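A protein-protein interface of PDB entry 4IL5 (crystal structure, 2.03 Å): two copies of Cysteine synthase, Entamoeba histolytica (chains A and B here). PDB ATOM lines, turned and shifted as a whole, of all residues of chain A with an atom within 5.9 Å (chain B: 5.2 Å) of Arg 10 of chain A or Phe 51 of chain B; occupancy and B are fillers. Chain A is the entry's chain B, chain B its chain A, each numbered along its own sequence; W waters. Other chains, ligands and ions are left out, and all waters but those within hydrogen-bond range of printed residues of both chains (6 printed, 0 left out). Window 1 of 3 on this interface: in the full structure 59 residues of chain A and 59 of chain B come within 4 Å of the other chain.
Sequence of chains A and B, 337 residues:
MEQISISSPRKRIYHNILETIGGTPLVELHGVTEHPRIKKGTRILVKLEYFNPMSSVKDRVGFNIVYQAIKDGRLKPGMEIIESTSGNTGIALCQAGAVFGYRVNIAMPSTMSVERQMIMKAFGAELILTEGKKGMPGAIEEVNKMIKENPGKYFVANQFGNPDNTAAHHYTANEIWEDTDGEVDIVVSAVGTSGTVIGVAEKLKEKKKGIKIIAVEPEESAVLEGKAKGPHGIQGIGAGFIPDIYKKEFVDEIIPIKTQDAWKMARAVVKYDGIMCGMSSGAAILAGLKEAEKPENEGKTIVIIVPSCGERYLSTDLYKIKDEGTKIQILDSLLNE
Of the 13 printed residues of chain A, 12 touch a printed residue of chain B. Hydrophobic or aromatic side chains of chain A within 4 Å of the printed part of chain B: Pro 9, Tyr 14, Ile 17, Phe 51 and Pro 53. Hydrophobic or aromatic side chains of chain B that line the printed part of chain A: Pro 25, Leu 48, Tyr 50, Phe 51 and Pro 53. Among the printed residues, 26 pairs touch across the chains.
The side-chain hydroxyl (OG1) of Thr 24 of chain B lies within hydrogen-bond range of the side-chain carboxylate (OE2) of Glu 49 of chain B. O of Pro 25 of chain B sits at hydrogen-bond distance from N of Leu 48 of chain B (3.0 Å). The guanidinium group of Arg 10 of chain A sits at hydrogen-bond distance from the side-chain hydroxyl of Tyr 14 of chain A. The backbone carbonyl oxygen of Ile 17 of chain A is in hydrogen-bond range of the side-chain hydroxyl of Thr 20 of chain A (2.6 Å).
Pro 9 of chain A touches Asp 179 of chain B (CB to OD1, 3.8 Å). NE of Arg 10 of chain A touches N of Pro 25 of chain B (3.5 Å). N of Arg 10 of chain A touches OD1 of Asp 179 of chain B, at 3.6 Å. Arg 12 of chain A touches Ser 7 of chain B. Asp 179 of chain B touches Arg 12 of chain A (CB to O, 3.8 Å). Tyr 14 of chain A touches Ser 7 of chain B (CE1 to OG, 3.6 Å). OG1 of Thr 20 of chain A touches CZ of Phe 51 of chain B, 3.2 Å away. Arg 10 of chain B touches Phe 51 of chain A. Thr 20 of chain B touches Phe 51 of chain A. Pro 53 of chain A touches Phe 51 of chain B (CA to CZ, 3.8 Å).
Water W1 bridges the side-chain hydroxyl of Tyr 50 of chain B (2.5 Å) and the backbone carbonyl oxygen of Pro 53 of chain A (3.2 Å). Water W3 lies within hydrogen-bond range of OD2 of Asp 179 of chain B (2.7 Å), N of Arg 10 of chain A (2.8 Å) and O of Thr 24 of chain B (2.9 Å). Water W4 lies within hydrogen-bond range of NH1 of Arg 10 of chain A, OG of Ser 7 of chain B and O of Thr 20 of chain A. Water W2 lies within hydrogen-bond range of the guanidinium group (NH2) of Arg 10 of chain A (2.8 Å), the guanidinium group (NH2) of Arg 10 of chain B (2.8 Å) and the backbone carbonyl oxygen (O) of Phe 51 of chain B (3.5 Å). Water W5 lies within hydrogen-bond range of the backbone carbonyl oxygen of Arg 12 of chain A (2.8 Å) and the side-chain carboxylate of Asp 179 of chain B (2.9 Å). Water W6 bridges NH2 of Arg 10 of chain A and NH2 of Arg 10 of chain B.
Arg 10 of chain A touches Phe 51 of chain B, and with the chains exchanged Phe 51 of chain A touches Arg 10 of chain B. Thr 20 of chain A touches Phe 51 of chain B, and with the chains exchanged Phe 51 of chain A touches Thr 20 of chain B. Phe 51 of chain B touches its own counterpart, Phe 51 of chain A. Phe 51 of chain A touches Pro 53 of chain B, and with the chains exchanged Pro 53 of chain A touches Phe 51 of chain B.
The backbone carbonyl oxygen (O) of Ile 21 of chain A sits at hydrogen-bond distance from the backbone NH (N) of Ser 7 of chain B. The guanidinium group (NE) of Arg 10 of chain B lies within hydrogen-bond range of the backbone carbonyl oxygen (O) of Gly 23 of chain A, at 2.8 Å. The backbone carbonyl oxygen (O) of Gly 23 of chain B sits at hydrogen-bond distance from the guanidinium group (NE) of Arg 10 of chain A. OD1 of Asp 179 of chain B sits at hydrogen-bond distance from N of Lys 11 of chain A (2.8 Å).
Printed residues of chain B within 4 Å of Arg 10 of chain A: Arg 10 (3.5 Å), Gly 23 (2.7 Å), Thr 24 (3.7 Å), Pro 25 (3.5 Å), Phe 51 (3.6 Å) and Asp 179 (3.6 Å). Printed residues of chain B within 4 Å of Lys 11 of chain A: Asp 179. Of the printed residues of chain A, Thr 20 of chain B touches Phe 51. Printed residues of chain A within 4 Å of Pro 25 of chain B: Arg 10 (3.5 Å), Tyr 14 (3.6 Å) and Thr 20 (3.9 Å). Glu 49 of chain B touches none of the printed residues of chain A. Of the printed residues of chain A, Tyr 50 of chain B touches Pro 53. Phe 51 of chain B touches just these residues of chain A: Arg 10 (3.6 Å), Thr 20 (3.2 Å), Phe 51 (3.4 Å) and Pro 53 (3.8 Å). Ser 55 of chain B touches none of the printed residues of chain A. The nearest residue of chain B that does not touch Arg 10 of chain A is Ser 7 of chain B (4.2 Å). The nearest printed residue of chain B that does not touch Lys 11 of chain A is Thr 24 of chain B (7.0 Å).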
ATOM      1  N   SER A   8       3.636 -34.133 -26.070  1.00  0.00           N
ATOM      2  CA  SER A   8       4.626 -33.320 -26.764  1.00  0.00           C
ATOM      3  C   SER A   8       4.078 -31.943 -27.051  1.00  0.00           C
ATOM      4  O   SER A   8       2.867 -31.755 -26.984  1.00  0.00           O
ATOM      5  CB  SER A   8       4.931 -33.960 -28.124  1.00  0.00           C
ATOM      6  OG  SER A   8       5.771 -35.063 -27.896  1.00  0.00           O
ATOM      7  N   PRO A   9       4.956 -30.996 -27.415  1.00  0.00           N
ATOM      8  CA  PRO A   9       4.467 -29.669 -27.752  1.00  0.00           C
ATOM      9  C   PRO A   9       3.448 -29.758 -28.883  1.00  0.00           C
ATOM     10  O   PRO A   9       3.551 -30.643 -29.739  1.00  0.00           O
ATOM     11  CB  PRO A   9       5.731 -28.941 -28.217  1.00  0.00           C
ATOM     12  CG  PRO A   9       6.848 -29.603 -27.431  1.00  0.00           C
ATOM     13  CD  PRO A   9       6.444 -31.062 -27.436  1.00  0.00           C
ATOM     14  N   ARG A  10       2.480 -28.850 -28.899  1.00  0.00           N
ATOM     15  CA  ARG A  10       1.514 -28.781 -30.014  1.00  0.00           C
ATOM     16  C   ARG A  10       2.123 -28.254 -31.331  1.00  0.00           C
ATOM     17  O   ARG A  10       1.626 -28.560 -32.427  1.00  0.00           O
ATOM     18  CB  ARG A  10       0.326 -27.905 -29.596  1.00  0.00           C
ATOM     19  CG  ARG A  10      -0.590 -28.577 -28.567  1.00  0.00           C
ATOM     20  CD  ARG A  10      -1.446 -27.565 -27.795  1.00  0.00           C
ATOM     21  NE  ARG A  10      -2.388 -28.247 -26.900  1.00  0.00           N
ATOM     22  CZ  ARG A  10      -3.702 -28.371 -27.115  1.00  0.00           C
ATOM     23  NH1 ARG A  10      -4.259 -27.839 -28.207  1.00  0.00           N
ATOM     24  NH2 ARG A  10      -4.470 -29.030 -26.232  1.00  0.00           N
ATOM     25  N   LYS A  11       3.187 -27.474 -31.226  1.00  0.00           N
ATOM     26  CA  LYS A  11       3.827 -26.828 -32.403  1.00  0.00           C
ATOM     27  C   LYS A  11       2.802 -26.014 -33.201  1.00  0.00           C
ATOM     28  O   LYS A  11       2.723 -26.132 -34.415  1.00  0.00           O
ATOM     29  CB  LYS A  11       4.521 -27.855 -33.323  1.00  0.00           C
ATOM     30  CG  LYS A  11       5.581 -28.732 -32.656  1.00  0.00           C
ATOM     31  CD  LYS A  11       6.166 -29.761 -33.624  1.00  0.00           C
ATOM     32  CE  LYS A  11       5.077 -30.725 -34.120  1.00  0.00           C
ATOM     33  NZ  LYS A  11       5.427 -31.537 -35.335  1.00  0.00           N
ATOM     34  N   ARG A  12       1.988 -25.234 -32.494  1.00  0.00           N
ATOM     35  CA  ARG A  12       0.996 -24.344 -33.112  1.00  0.00           C
ATOM     36  C   ARG A  12       0.914 -23.143 -32.179  1.00  0.00           C
ATOM     37  O   ARG A  12       1.171 -23.273 -30.968  1.00  0.00           O
ATOM     38  CB  ARG A  12      -0.397 -25.012 -33.273  1.00  0.00           C
ATOM     39  CG  ARG A  12      -1.398 -24.170 -34.115  1.00  0.00           C
ATOM     40  CD  ARG A  12      -2.652 -24.896 -34.614  1.00  0.00           C
ATOM     41  NE  ARG A  12      -3.650 -23.962 -35.183  1.00  0.00           N
ATOM     42  CZ  ARG A  12      -4.959 -24.210 -35.329  1.00  0.00           C
ATOM     43  NH1 ARG A  12      -5.505 -25.375 -34.941  1.00  0.00           N
ATOM     44  NH2 ARG A  12      -5.746 -23.281 -35.865  1.00  0.00           N
ATOM     45  N   TYR A  14      -2.165 -20.700 -31.516  1.00  0.00           N
ATOM     46  CA  TYR A  14      -3.578 -20.527 -31.794  1.00  0.00           C
ATOM     47  C   TYR A  14      -3.908 -19.035 -31.855  1.00  0.00           C
ATOM     48  O   TYR A  14      -3.419 -18.246 -31.031  1.00  0.00           O
ATOM     49  CB  TYR A  14      -4.426 -21.261 -30.733  1.00  0.00           C
ATOM     50  CG  TYR A  14      -4.066 -22.718 -30.669  1.00  0.00           C
ATOM     51  CD1 TYR A  14      -4.775 -23.654 -31.408  1.00  0.00           C
ATOM     52  CD2 TYR A  14      -2.970 -23.153 -29.926  1.00  0.00           C
ATOM     53  CE1 TYR A  14      -4.437 -24.991 -31.384  1.00  0.00           C
ATOM     54  CE2 TYR A  14      -2.607 -24.489 -29.907  1.00  0.00           C
ATOM     55  CZ  TYR A  14      -3.349 -25.401 -30.648  1.00  0.00           C
ATOM     56  OH  TYR A  14      -3.017 -26.735 -30.647  1.00  0.00           O
ATOM     57  N   ILE A  17      -9.025 -18.504 -28.688  1.00  0.00           N
ATOM     58  CA  ILE A  17      -9.368 -19.679 -27.888  1.00  0.00           C
ATOM     59  C   ILE A  17     -10.196 -20.734 -28.668  1.00  0.00           C
ATOM     60  O   ILE A  17     -10.148 -21.936 -28.331  1.00  0.00           O
ATOM     61  CB  ILE A  17     -10.079 -19.259 -26.550  1.00  0.00           C
ATOM     62  CG1 ILE A  17     -10.145 -20.426 -25.549  1.00  0.00           C
ATOM     63  CG2 ILE A  17     -11.437 -18.615 -26.797  1.00  0.00           C
ATOM     64  CD1 ILE A  17      -8.783 -20.800 -24.999  1.00  0.00           C
ATOM     65  N   THR A  20      -8.570 -23.744 -30.190  1.00  0.00           N
ATOM     66  CA  THR A  20      -8.188 -24.863 -29.285  1.00  0.00           C
ATOM     67  C   THR A  20      -9.335 -25.835 -29.040  1.00  0.00           C
ATOM     68  O   THR A  20      -9.178 -26.823 -28.316  1.00  0.00           O
ATOM     69  CB  THR A  20      -7.690 -24.377 -27.907  1.00  0.00           C
ATOM     70  OG1 THR A  20      -8.806 -23.874 -27.145  1.00  0.00           O
ATOM     71  CG2 THR A  20      -6.587 -23.305 -28.059  1.00  0.00           C
ATOM     72  N   ILE A  21     -10.506 -25.549 -29.623  1.00  0.00           N
ATOM     73  CA  ILE A  21     -11.626 -26.482 -29.594  1.00  0.00           C
ATOM     74  C   ILE A  21     -11.279 -27.738 -30.402  1.00  0.00           C
ATOM     75  O   ILE A  21     -10.628 -27.641 -31.431  1.00  0.00           O
ATOM     76  CB  ILE A  21     -12.920 -25.778 -30.102  1.00  0.00           C
ATOM     77  CG1 ILE A  21     -13.376 -24.701 -29.071  1.00  0.00           C
ATOM     78  CG2 ILE A  21     -14.042 -26.780 -30.389  1.00  0.00           C
ATOM     79  CD1 ILE A  21     -14.479 -23.767 -29.578  1.00  0.00           C
ATOM     80  N   GLY A  23      -9.889 -31.856 -31.289  1.00  0.00           N
ATOM     81  CA  GLY A  23      -8.630 -32.611 -31.129  1.00  0.00           C
ATOM     82  C   GLY A  23      -8.503 -33.099 -29.685  1.00  0.00           C
ATOM     83  O   GLY A  23      -7.419 -33.002 -29.082  1.00  0.00           O
ATOM     84  N   PHE A  51     -11.552 -31.679 -22.400  1.00  0.00           N
ATOM     85  CA  PHE A  51     -10.298 -31.010 -22.802  1.00  0.00           C
ATOM     86  C   PHE A  51     -10.512 -29.741 -23.655  1.00  0.00           C
ATOM     87  O   PHE A  51      -9.578 -28.967 -23.881  1.00  0.00           O
ATOM     88  CB  PHE A  51      -9.329 -31.984 -23.511  1.00  0.00           C
ATOM     89  CG  PHE A  51      -8.486 -32.784 -22.557  1.00  0.00           C
ATOM     90  CD1 PHE A  51      -9.079 -33.721 -21.702  1.00  0.00           C
ATOM     91  CD2 PHE A  51      -7.104 -32.603 -22.512  1.00  0.00           C
ATOM     92  CE1 PHE A  51      -8.306 -34.459 -20.805  1.00  0.00           C
ATOM     93  CE2 PHE A  51      -6.314 -33.331 -21.624  1.00  0.00           C
ATOM     94  CZ  PHE A  51      -6.913 -34.262 -20.771  1.00  0.00           C
ATOM     95  N   ASN A  52     -11.723 -29.561 -24.163  1.00  0.00           N
ATOM     96  CA  ASN A  52     -12.151 -28.299 -24.786  1.00  0.00           C
ATOM     97  C   ASN A  52     -11.965 -27.100 -23.841  1.00  0.00           C
ATOM     98  O   ASN A  52     -12.000 -27.260 -22.638  1.00  0.00           O
ATOM     99  CB  ASN A  52     -13.622 -28.418 -25.196  1.00  0.00           C
ATOM    100  CG  ASN A  52     -13.802 -29.235 -26.464  1.00  0.00           C
ATOM    101  OD1 ASN A  52     -14.551 -30.238 -26.498  1.00  0.00           O
ATOM    102  ND2 ASN A  52     -13.072 -28.864 -27.487  1.00  0.00           N
ATOM    103  N   PRO A  53     -11.818 -25.879 -24.390  1.00  0.00           N
ATOM    104  CA  PRO A  53     -11.480 -24.725 -23.519  1.00  0.00           C
ATOM    105  C   PRO A  53     -12.445 -24.440 -22.385  1.00  0.00           C
ATOM    106  O   PRO A  53     -11.992 -24.036 -21.310  1.00  0.00           O
ATOM    107  CB  PRO A  53     -11.398 -23.537 -24.497  1.00  0.00           C
ATOM    108  CG  PRO A  53     -11.967 -24.037 -25.789  1.00  0.00           C
ATOM    109  CD  PRO A  53     -11.724 -25.524 -25.809  1.00  0.00           C
ATOM    110  N   SER B   7      -8.758 -27.476 -33.714  1.00  0.00           N
ATOM    111  CA  SER B   7      -7.607 -28.361 -33.567  1.00  0.00           C
ATOM    112  C   SER B   7      -7.744 -29.654 -34.341  1.00  0.00           C
ATOM    113  O   SER B   7      -8.824 -30.259 -34.377  1.00  0.00           O
ATOM    114  CB  SER B   7      -7.377 -28.705 -32.098  1.00  0.00           C
ATOM    115  OG  SER B   7      -7.004 -27.550 -31.381  1.00  0.00           O
ATOM    116  N   ARG B  10      -5.252 -35.580 -32.371  1.00  0.00           N
ATOM    117  CA  ARG B  10      -3.963 -35.781 -31.709  1.00  0.00           C
ATOM    118  C   ARG B  10      -3.145 -36.896 -32.377  1.00  0.00           C
ATOM    119  O   ARG B  10      -1.922 -36.876 -32.297  1.00  0.00           O
ATOM    120  CB  ARG B  10      -4.186 -36.089 -30.217  1.00  0.00           C
ATOM    121  CG  ARG B  10      -4.389 -34.844 -29.351  1.00  0.00           C
ATOM    122  CD  ARG B  10      -5.183 -35.170 -28.103  1.00  0.00           C
ATOM    123  NE  ARG B  10      -5.479 -33.943 -27.344  1.00  0.00           N
ATOM    124  CZ  ARG B  10      -4.787 -33.565 -26.278  1.00  0.00           C
ATOM    125  NH1 ARG B  10      -3.784 -34.332 -25.878  1.00  0.00           N
ATOM    126  NH2 ARG B  10      -5.091 -32.443 -25.621  1.00  0.00           N
ATOM    127  N   THR B  20      -1.711 -37.401 -20.904  1.00  0.00           N
ATOM    128  CA  THR B  20      -2.327 -36.188 -21.484  1.00  0.00           C
ATOM    129  C   THR B  20      -1.873 -34.896 -20.785  1.00  0.00           C
ATOM    130  O   THR B  20      -2.324 -33.790 -21.145  1.00  0.00           O
ATOM    131  CB  THR B  20      -3.859 -36.212 -21.418  1.00  0.00           C
ATOM    132  OG1 THR B  20      -4.262 -36.168 -20.051  1.00  0.00           O
ATOM    133  CG2 THR B  20      -4.406 -37.478 -22.065  1.00  0.00           C
ATOM    134  N   GLY B  23       2.061 -30.312 -23.015  1.00  0.00           N
ATOM    135  CA  GLY B  23       1.703 -29.966 -24.412  1.00  0.00           C
ATOM    136  C   GLY B  23       0.484 -29.054 -24.429  1.00  0.00           C
ATOM    137  O   GLY B  23      -0.457 -29.221 -25.226  1.00  0.00           O
ATOM    138  N   THR B  24       0.520 -28.044 -23.568  1.00  0.00           N
ATOM    139  CA  THR B  24      -0.612 -27.129 -23.466  1.00  0.00           C
ATOM    140  C   THR B  24      -0.548 -26.014 -24.519  1.00  0.00           C
ATOM    141  O   THR B  24       0.537 -25.679 -25.011  1.00  0.00           O
ATOM    142  CB  THR B  24      -0.673 -26.505 -22.062  1.00  0.00           C
ATOM    143  OG1 THR B  24       0.570 -25.860 -21.786  1.00  0.00           O
ATOM    144  CG2 THR B  24      -0.975 -27.580 -20.992  1.00  0.00           C
ATOM    145  N   PRO B  25      -1.719 -25.434 -24.875  1.00  0.00           N
ATOM    146  CA  PRO B  25      -1.753 -24.524 -26.027  1.00  0.00           C
ATOM    147  C   PRO B  25      -1.266 -23.103 -25.727  1.00  0.00           C
ATOM    148  O   PRO B  25      -1.474 -22.542 -24.618  1.00  0.00           O
ATOM    149  CB  PRO B  25      -3.233 -24.489 -26.410  1.00  0.00           C
ATOM    150  CG  PRO B  25      -3.969 -24.804 -25.132  1.00  0.00           C
ATOM    151  CD  PRO B  25      -3.071 -25.721 -24.342  1.00  0.00           C
ATOM    152  N   LEU B  48      -1.937 -21.946 -21.728  1.00  0.00           N
ATOM    153  CA  LEU B  48      -3.115 -22.244 -20.935  1.00  0.00           C
ATOM    154  C   LEU B  48      -2.927 -23.571 -20.220  1.00  0.00           C
ATOM    155  O   LEU B  48      -3.204 -24.639 -20.763  1.00  0.00           O
ATOM    156  CB  LEU B  48      -4.374 -22.219 -21.845  1.00  0.00           C
ATOM    157  CG  LEU B  48      -4.603 -20.931 -22.641  1.00  0.00           C
ATOM    158  CD1 LEU B  48      -5.897 -21.033 -23.467  1.00  0.00           C
ATOM    159  CD2 LEU B  48      -4.692 -19.703 -21.715  1.00  0.00           C
ATOM    160  N   GLU B  49      -2.462 -23.497 -18.980  1.00  0.00           N
ATOM    161  CA  GLU B  49      -2.125 -24.702 -18.222  1.00  0.00           C
ATOM    162  C   GLU B  49      -3.342 -25.423 -17.664  1.00  0.00           C
ATOM    163  O   GLU B  49      -3.224 -26.562 -17.180  1.00  0.00           O
ATOM    164  CB  GLU B  49      -1.129 -24.383 -17.099  1.00  0.00           C
ATOM    165  CG  GLU B  49       0.252 -24.039 -17.621  1.00  0.00           C
ATOM    166  CD  GLU B  49       0.871 -25.257 -18.258  1.00  0.00           C
ATOM    167  OE1 GLU B  49       0.755 -26.349 -17.666  1.00  0.00           O
ATOM    168  OE2 GLU B  49       1.441 -25.122 -19.360  1.00  0.00           O
ATOM    169  N   TYR B  50      -4.509 -24.787 -17.743  1.00  0.00           N
ATOM    170  CA  TYR B  50      -5.753 -25.490 -17.459  1.00  0.00           C
ATOM    171  C   TYR B  50      -6.170 -26.521 -18.545  1.00  0.00           C
ATOM    172  O   TYR B  50      -7.130 -27.247 -18.351  1.00  0.00           O
ATOM    173  CB  TYR B  50      -6.907 -24.532 -17.097  1.00  0.00           C
ATOM    174  CG  TYR B  50      -7.321 -23.523 -18.166  1.00  0.00           C
ATOM    175  CD1 TYR B  50      -6.856 -22.192 -18.132  1.00  0.00           C
ATOM    176  CD2 TYR B  50      -8.240 -23.875 -19.146  1.00  0.00           C
ATOM    177  CE1 TYR B  50      -7.270 -21.267 -19.073  1.00  0.00           C
ATOM    178  CE2 TYR B  50      -8.676 -22.957 -20.088  1.00  0.00           C
ATOM    179  CZ  TYR B  50      -8.194 -21.671 -20.045  1.00  0.00           C
ATOM    180  OH  TYR B  50      -8.641 -20.784 -20.969  1.00  0.00           O
ATOM    181  N   PHE B  51      -5.418 -26.625 -19.644  1.00  0.00           N
ATOM    182  CA  PHE B  51      -5.656 -27.733 -20.595  1.00  0.00           C
ATOM    183  C   PHE B  51      -5.154 -29.078 -20.072  1.00  0.00           C
ATOM    184  O   PHE B  51      -5.505 -30.128 -20.595  1.00  0.00           O
ATOM    185  CB  PHE B  51      -5.101 -27.422 -21.989  1.00  0.00           C
ATOM    186  CG  PHE B  51      -6.057 -26.599 -22.830  1.00  0.00           C
ATOM    187  CD1 PHE B  51      -6.369 -25.278 -22.458  1.00  0.00           C
ATOM    188  CD2 PHE B  51      -6.619 -27.129 -23.980  1.00  0.00           C
ATOM    189  CE1 PHE B  51      -7.238 -24.497 -23.220  1.00  0.00           C
ATOM    190  CE2 PHE B  51      -7.499 -26.361 -24.743  1.00  0.00           C
ATOM    191  CZ  PHE B  51      -7.803 -25.042 -24.357  1.00  0.00           C
ATOM    192  N   ASN B  52      -4.362 -29.045 -19.005  1.00  0.00           N
ATOM    193  CA  ASN B  52      -4.000 -30.279 -18.262  1.00  0.00           C
ATOM    194  C   ASN B  52      -5.252 -31.030 -17.793  1.00  0.00           C
ATOM    195  O   ASN B  52      -6.299 -30.406 -17.630  1.00  0.00           O
ATOM    196  CB  ASN B  52      -3.093 -29.899 -17.075  1.00  0.00           C
ATOM    197  CG  ASN B  52      -1.688 -29.603 -17.529  1.00  0.00           C
ATOM    198  OD1 ASN B  52      -1.165 -28.485 -17.369  1.00  0.00           O
ATOM    199  ND2 ASN B  52      -1.061 -30.608 -18.125  1.00  0.00           N
ATOM    200  N   PRO B  53      -5.160 -32.363 -17.576  1.00  0.00           N
ATOM    201  CA  PRO B  53      -6.420 -33.109 -17.313  1.00  0.00           C
ATOM    202  C   PRO B  53      -7.219 -32.677 -16.072  1.00  0.00           C
ATOM    203  O   PRO B  53      -8.438 -32.847 -16.063  1.00  0.00           O
ATOM    204  CB  PRO B  53      -5.970 -34.560 -17.165  1.00  0.00           C
ATOM    205  CG  PRO B  53      -4.452 -34.535 -17.044  1.00  0.00           C
ATOM    206  CD  PRO B  53      -4.021 -33.281 -17.796  1.00  0.00           C
ATOM    207  N   SER B  55      -6.914 -29.507 -14.973  1.00  0.00           N
ATOM    208  CA  SER B  55      -7.153 -28.074 -15.147  1.00  0.00           C
ATOM    209  C   SER B  55      -6.216 -27.127 -14.389  1.00  0.00           C
ATOM    210  O   SER B  55      -6.554 -25.960 -14.143  1.00  0.00           O
ATOM    211  CB  SER B  55      -8.639 -27.743 -14.897  1.00  0.00           C
ATOM    212  OG  SER B  55      -9.454 -28.445 -15.858  1.00  0.00           O
ATOM    213  N   ASP B 179       6.782 -24.104 -29.696  1.00  0.00           N
ATOM    214  CA  ASP B 179       5.583 -23.478 -30.174  1.00  0.00           C
ATOM    215  C   ASP B 179       5.846 -22.115 -30.791  1.00  0.00           C
ATOM    216  O   ASP B 179       5.159 -21.758 -31.684  1.00  0.00           O
ATOM    217  CB  ASP B 179       4.508 -23.377 -29.112  1.00  0.00           C
ATOM    218  CG  ASP B 179       3.931 -24.710 -28.718  1.00  0.00           C
ATOM    219  OD1 ASP B 179       4.199 -25.701 -29.336  1.00  0.00           O
ATOM    220  OD2 ASP B 179       3.206 -24.737 -27.782  1.00  0.00           O
HETATM  221  O   HOH W   1     -11.137 -20.952 -21.275  1.00  0.00           O
HETATM  222  O   HOH W   2      -4.227 -30.423 -23.832  1.00  0.00           O
HETATM  223  O   HOH W   3       2.507 -27.077 -26.700  1.00  0.00           O
HETATM  224  O   HOH W   4      -6.851 -28.307 -28.756  1.00  0.00           O
HETATM  225  O   HOH W   5       0.381 -24.387 -28.500  1.00  0.00           O
HETATM  226  O   HOH W   6      -7.112 -30.212 -26.045  1.00  0.00           O
